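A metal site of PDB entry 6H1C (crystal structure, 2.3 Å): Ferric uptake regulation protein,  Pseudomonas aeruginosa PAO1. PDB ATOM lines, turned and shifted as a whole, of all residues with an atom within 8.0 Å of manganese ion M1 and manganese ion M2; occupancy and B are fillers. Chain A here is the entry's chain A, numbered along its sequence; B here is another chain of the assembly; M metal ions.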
ATOM      1  N   SER A  34     -32.541  -8.547   7.005  1.00  0.00           N
ATOM      2  CA  SER A  34     -31.627  -9.163   6.040  1.00  0.00           C
ATOM      3  C   SER A  34     -32.127 -10.551   5.659  1.00  0.00           C
ATOM      4  O   SER A  34     -33.051 -11.099   6.269  1.00  0.00           O
ATOM      5  CB  SER A  34     -30.227  -9.282   6.623  1.00  0.00           C
ATOM      6  OG  SER A  34     -30.173 -10.317   7.578  1.00  0.00           O
ATOM      7  N   ASN A  71     -29.642  -1.158   0.392  1.00  0.00           N
ATOM      8  CA  ASN A  71     -28.328  -1.449   0.973  1.00  0.00           C
ATOM      9  C   ASN A  71     -27.906  -0.193   1.734  1.00  0.00           C
ATOM     10  O   ASN A  71     -27.313   0.710   1.153  1.00  0.00           O
ATOM     11  CB  ASN A  71     -27.324  -1.828  -0.095  1.00  0.00           C
ATOM     12  CG  ASN A  71     -26.031  -2.364   0.498  1.00  0.00           C
ATOM     13  OD1 ASN A  71     -25.403  -1.696   1.306  1.00  0.00           O
ATOM     14  ND2 ASN A  71     -25.667  -3.582   0.137  1.00  0.00           N
ATOM     15  N   PHE A  72     -28.217  -0.137   3.023  1.00  0.00           N
ATOM     16  CA  PHE A  72     -28.063   1.121   3.738  1.00  0.00           C
ATOM     17  C   PHE A  72     -26.630   1.333   4.187  1.00  0.00           C
ATOM     18  O   PHE A  72     -26.062   2.415   4.000  1.00  0.00           O
ATOM     19  CB  PHE A  72     -29.000   1.210   4.942  1.00  0.00           C
ATOM     20  CG  PHE A  72     -30.455   1.332   4.561  1.00  0.00           C
ATOM     21  CD1 PHE A  72     -30.895   2.403   3.824  1.00  0.00           C
ATOM     22  CD2 PHE A  72     -31.363   0.398   4.965  1.00  0.00           C
ATOM     23  CE1 PHE A  72     -32.213   2.531   3.487  1.00  0.00           C
ATOM     24  CE2 PHE A  72     -32.681   0.516   4.626  1.00  0.00           C
ATOM     25  CZ  PHE A  72     -33.101   1.588   3.887  1.00  0.00           C
ATOM     26  N   ASP A  73     -26.000   0.307   4.762  1.00  0.00           N
ATOM     27  CA  ASP A  73     -24.658   0.508   5.282  1.00  0.00           C
ATOM     28  C   ASP A  73     -23.574   0.022   4.342  1.00  0.00           C
ATOM     29  O   ASP A  73     -22.411  -0.025   4.742  1.00  0.00           O
ATOM     30  CB  ASP A  73     -24.513  -0.147   6.652  1.00  0.00           C
ATOM     31  CG  ASP A  73     -24.574  -1.645   6.605  1.00  0.00           C
ATOM     32  OD1 ASP A  73     -24.392  -2.244   5.515  1.00  0.00           O
ATOM     33  OD2 ASP A  73     -24.800  -2.227   7.688  1.00  0.00           O
ATOM     34  N   GLY A  74     -23.906  -0.310   3.091  1.00  0.00           N
ATOM     35  CA  GLY A  74     -22.935  -0.783   2.127  1.00  0.00           C
ATOM     36  C   GLY A  74     -22.665  -2.276   2.149  1.00  0.00           C
ATOM     37  O   GLY A  74     -22.222  -2.832   1.143  1.00  0.00           O
ATOM     38  N   GLY A  75     -22.944  -2.943   3.268  1.00  0.00           N
ATOM     39  CA  GLY A  75     -22.495  -4.304   3.457  1.00  0.00           C
ATOM     40  C   GLY A  75     -23.529  -5.389   3.237  1.00  0.00           C
ATOM     41  O   GLY A  75     -23.193  -6.433   2.699  1.00  0.00           O
ATOM     42  N   HIS A  76     -24.774  -5.178   3.644  1.00  0.00           N
ATOM     43  CA  HIS A  76     -25.782  -6.219   3.558  1.00  0.00           C
ATOM     44  C   HIS A  76     -27.084  -5.665   2.980  1.00  0.00           C
ATOM     45  O   HIS A  76     -27.381  -4.471   3.075  1.00  0.00           O
ATOM     46  CB  HIS A  76     -26.042  -6.867   4.911  1.00  0.00           C
ATOM     47  CG  HIS A  76     -27.036  -6.145   5.749  1.00  0.00           C
ATOM     48  ND1 HIS A  76     -26.709  -5.053   6.520  1.00  0.00           N
ATOM     49  CD2 HIS A  76     -28.352  -6.375   5.974  1.00  0.00           C
ATOM     50  CE1 HIS A  76     -27.779  -4.629   7.165  1.00  0.00           C
ATOM     51  NE2 HIS A  76     -28.794  -5.418   6.850  1.00  0.00           N
ATOM     52  N   ALA A  77     -27.841  -6.562   2.362  1.00  0.00           N
ATOM     53  CA  ALA A  77     -29.087  -6.208   1.699  1.00  0.00           C
ATOM     54  C   ALA A  77     -30.240  -6.235   2.692  1.00  0.00           C
ATOM     55  O   ALA A  77     -30.349  -7.153   3.511  1.00  0.00           O
ATOM     56  CB  ALA A  77     -29.379  -7.156   0.534  1.00  0.00           C
ATOM     57  N   VAL A  78     -31.100  -5.226   2.603  1.00  0.00           N
ATOM     58  CA  VAL A  78     -32.297  -5.102   3.439  1.00  0.00           C
ATOM     59  C   VAL A  78     -33.521  -5.336   2.573  1.00  0.00           C
ATOM     60  O   VAL A  78     -33.667  -4.731   1.502  1.00  0.00           O
ATOM     61  CB  VAL A  78     -32.390  -3.694   4.074  1.00  0.00           C
ATOM     62  CG1 VAL A  78     -33.846  -3.380   4.440  1.00  0.00           C
ATOM     63  CG2 VAL A  78     -31.481  -3.602   5.288  1.00  0.00           C
ATOM     64  N   THR A  95     -23.600   4.487  13.224  1.00  0.00           N
ATOM     65  CA  THR A  95     -24.123   3.262  13.804  1.00  0.00           C
ATOM     66  C   THR A  95     -24.878   2.374  12.820  1.00  0.00           C
ATOM     67  O   THR A  95     -25.030   1.187  13.081  1.00  0.00           O
ATOM     68  CB  THR A  95     -25.053   3.589  14.967  1.00  0.00           C
ATOM     69  OG1 THR A  95     -26.167   4.363  14.494  1.00  0.00           O
ATOM     70  CG2 THR A  95     -24.303   4.373  16.049  1.00  0.00           C
ATOM     71  N   GLY A  96     -25.342   2.912  11.691  1.00  0.00           N
ATOM     72  CA  GLY A  96     -26.254   2.174  10.850  1.00  0.00           C
ATOM     73  C   GLY A  96     -27.684   2.160  11.342  1.00  0.00           C
ATOM     74  O   GLY A  96     -28.492   1.380  10.828  1.00  0.00           O
ATOM     75  N   SER B  34     -18.337  -9.805   8.052  1.00  0.00           N
ATOM     76  CA  SER B  34     -19.089  -8.700   7.483  1.00  0.00           C
ATOM     77  C   SER B  34     -18.501  -7.356   7.908  1.00  0.00           C
ATOM     78  O   SER B  34     -17.709  -7.258   8.843  1.00  0.00           O
ATOM     79  CB  SER B  34     -20.541  -8.781   7.939  1.00  0.00           C
ATOM     80  OG  SER B  34     -20.682  -8.261   9.247  1.00  0.00           O
ATOM     81  N   ALA B  35     -18.898  -6.298   7.194  1.00  0.00           N
ATOM     82  CA  ALA B  35     -18.527  -4.962   7.657  1.00  0.00           C
ATOM     83  C   ALA B  35     -19.039  -4.714   9.069  1.00  0.00           C
ATOM     84  O   ALA B  35     -18.370  -4.076   9.879  1.00  0.00           O
ATOM     85  CB  ALA B  35     -19.066  -3.903   6.697  1.00  0.00           C
ATOM     86  N   GLU B  36     -20.235  -5.205   9.377  1.00  0.00           N
ATOM     87  CA  GLU B  36     -20.783  -5.049  10.721  1.00  0.00           C
ATOM     88  C   GLU B  36     -19.942  -5.790  11.753  1.00  0.00           C
ATOM     89  O   GLU B  36     -19.725  -5.289  12.859  1.00  0.00           O
ATOM     90  CB  GLU B  36     -22.236  -5.528  10.759  1.00  0.00           C
ATOM     91  CG  GLU B  36     -23.291  -4.478  10.498  1.00  0.00           C
ATOM     92  CD  GLU B  36     -24.699  -4.991  10.799  1.00  0.00           C
ATOM     93  OE1 GLU B  36     -25.024  -5.244  11.979  1.00  0.00           O
ATOM     94  OE2 GLU B  36     -25.471  -5.168   9.851  1.00  0.00           O
ATOM     95  N   ASP B  37     -19.455  -6.989  11.409  1.00  0.00           N
ATOM     96  CA  ASP B  37     -18.552  -7.721  12.302  1.00  0.00           C
ATOM     97  C   ASP B  37     -17.304  -6.920  12.628  1.00  0.00           C
ATOM     98  O   ASP B  37     -16.825  -6.944  13.762  1.00  0.00           O
ATOM     99  CB  ASP B  37     -18.137  -9.035  11.677  1.00  0.00           C
ATOM    100  CG  ASP B  37     -19.283  -9.983  11.480  1.00  0.00           C
ATOM    101  OD1 ASP B  37     -20.279  -9.845  12.241  1.00  0.00           O
ATOM    102  OD2 ASP B  37     -19.179 -10.861  10.588  1.00  0.00           O
ATOM    103  N   LYS B  40     -18.409  -4.014  15.009  1.00  0.00           N
ATOM    104  CA  LYS B  40     -18.634  -4.540  16.353  1.00  0.00           C
ATOM    105  C   LYS B  40     -17.306  -4.864  17.030  1.00  0.00           C
ATOM    106  O   LYS B  40     -17.088  -4.491  18.189  1.00  0.00           O
ATOM    107  CB  LYS B  40     -19.531  -5.776  16.299  1.00  0.00           C
ATOM    108  CG  LYS B  40     -20.868  -5.540  15.602  1.00  0.00           C
ATOM    109  CD  LYS B  40     -21.831  -6.763  15.670  1.00  0.00           C
ATOM    110  CE  LYS B  40     -23.149  -6.485  14.894  1.00  0.00           C
ATOM    111  NZ  LYS B  40     -24.109  -7.621  14.841  1.00  0.00           N
ATOM    112  N   LEU B  51     -19.445   2.936  11.432  1.00  0.00           N
ATOM    113  CA  LEU B  51     -19.765   1.926  10.426  1.00  0.00           C
ATOM    114  C   LEU B  51     -19.457   2.421   9.016  1.00  0.00           C
ATOM    115  O   LEU B  51     -18.894   1.681   8.193  1.00  0.00           O
ATOM    116  CB  LEU B  51     -21.239   1.555  10.562  1.00  0.00           C
ATOM    117  CG  LEU B  51     -21.783   0.406   9.740  1.00  0.00           C
ATOM    118  CD1 LEU B  51     -20.888  -0.794   9.901  1.00  0.00           C
ATOM    119  CD2 LEU B  51     -23.185   0.091  10.220  1.00  0.00           C
ATOM    120  N   TYR B  55     -16.758   0.506   6.403  1.00  0.00           N
ATOM    121  CA  TYR B  55     -17.046   0.015   5.064  1.00  0.00           C
ATOM    122  C   TYR B  55     -16.160   0.680   4.027  1.00  0.00           C
ATOM    123  O   TYR B  55     -15.683   0.013   3.103  1.00  0.00           O
ATOM    124  CB  TYR B  55     -18.516   0.240   4.739  1.00  0.00           C
ATOM    125  CG  TYR B  55     -18.844  -0.164   3.346  1.00  0.00           C
ATOM    126  CD1 TYR B  55     -18.958  -1.511   3.000  1.00  0.00           C
ATOM    127  CD2 TYR B  55     -19.041   0.783   2.357  1.00  0.00           C
ATOM    128  CE1 TYR B  55     -19.245  -1.896   1.696  1.00  0.00           C
ATOM    129  CE2 TYR B  55     -19.316   0.397   1.061  1.00  0.00           C
ATOM    130  CZ  TYR B  55     -19.418  -0.933   0.736  1.00  0.00           C
ATOM    131  OH  TYR B  55     -19.713  -1.300  -0.555  1.00  0.00           O
ATOM    132  N   GLY B  75     -26.697 -12.071   0.213  1.00  0.00           N
ATOM    133  CA  GLY B  75     -27.336 -11.023   0.985  1.00  0.00           C
ATOM    134  C   GLY B  75     -26.415 -10.117   1.776  1.00  0.00           C
ATOM    135  O   GLY B  75     -26.853  -9.054   2.239  1.00  0.00           O
ATOM    136  N   HIS B  76     -25.141 -10.495   1.944  1.00  0.00           N
ATOM    137  CA  HIS B  76     -24.203  -9.615   2.628  1.00  0.00           C
ATOM    138  C   HIS B  76     -22.792  -9.916   2.157  1.00  0.00           C
ATOM    139  O   HIS B  76     -22.464 -11.041   1.772  1.00  0.00           O
ATOM    140  CB  HIS B  76     -24.315  -9.750   4.161  1.00  0.00           C
ATOM    141  CG  HIS B  76     -23.538 -10.888   4.753  1.00  0.00           C
ATOM    142  ND1 HIS B  76     -24.063 -12.159   4.919  1.00  0.00           N
ATOM    143  CD2 HIS B  76     -22.266 -10.953   5.217  1.00  0.00           C
ATOM    144  CE1 HIS B  76     -23.144 -12.943   5.447  1.00  0.00           C
ATOM    145  NE2 HIS B  76     -22.051 -12.247   5.638  1.00  0.00           N
ATOM    146  N   ALA B  77     -21.939  -8.903   2.208  1.00  0.00           N
ATOM    147  CA  ALA B  77     -20.575  -8.982   1.732  1.00  0.00           C
ATOM    148  C   ALA B  77     -19.633  -9.488   2.823  1.00  0.00           C
ATOM    149  O   ALA B  77     -19.718  -9.089   3.985  1.00  0.00           O
ATOM    150  CB  ALA B  77     -20.118  -7.626   1.220  1.00  0.00           C
HETATM  151 MN    MN M   1     -24.753  -4.622   7.875  1.00  0.00          MN
HETATM  152 MN    MN M   2     -24.847  -4.332   7.050  1.00  0.00          MN
HETATM  153 MN    MN M   3     -22.852  -5.692   6.790  1.00  0.00          MN
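The side-chain hydroxyl (OG) of Ser 34 of chain B is in hydrogen-bond range of the backbone NH (N) of Glu 36 of chain B, at 3.1 Å.
The side-chain carboxylate (OE1) of Glu 36 of chain B is in salt-bridge range of the side-chain amino group (NZ) of Lys 40 of chain B (3.8 Å).
The side-chain carboxylate (OD1) of Asp 73 lies close to the backbone NH (N) of Gly 75 of chain A, at 2.8 Å.
Within 4 Å of manganese ion M1: Asp 73, His 76 of chain A and Glu 36 of chain B.
Along chain A the residues within 4 Å of manganese ion M1 span positions 73 to 76.
Three residues have an atom within 4 Å of manganese ion M2: Asp 73, His 76 of chain A and Glu 36 of chain B.
The nearest printed residue that does not touch manganese ion M2 is Gly 75 of chain A (4.2 Å).
Manganese ion M1 is bound by OE2 of Glu 36 of chain B (2.2 Å), OD2 of Asp 73 (2.4 Å) and ND1 of His 76 of chain A (2.4 Å).
Manganese ion M2 is bound by ND1 of His 76 of chain A (2.1 Å), OD2 of Asp 73 (2.2 Å) and OD1 of Asp 73 (2.6 Å).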
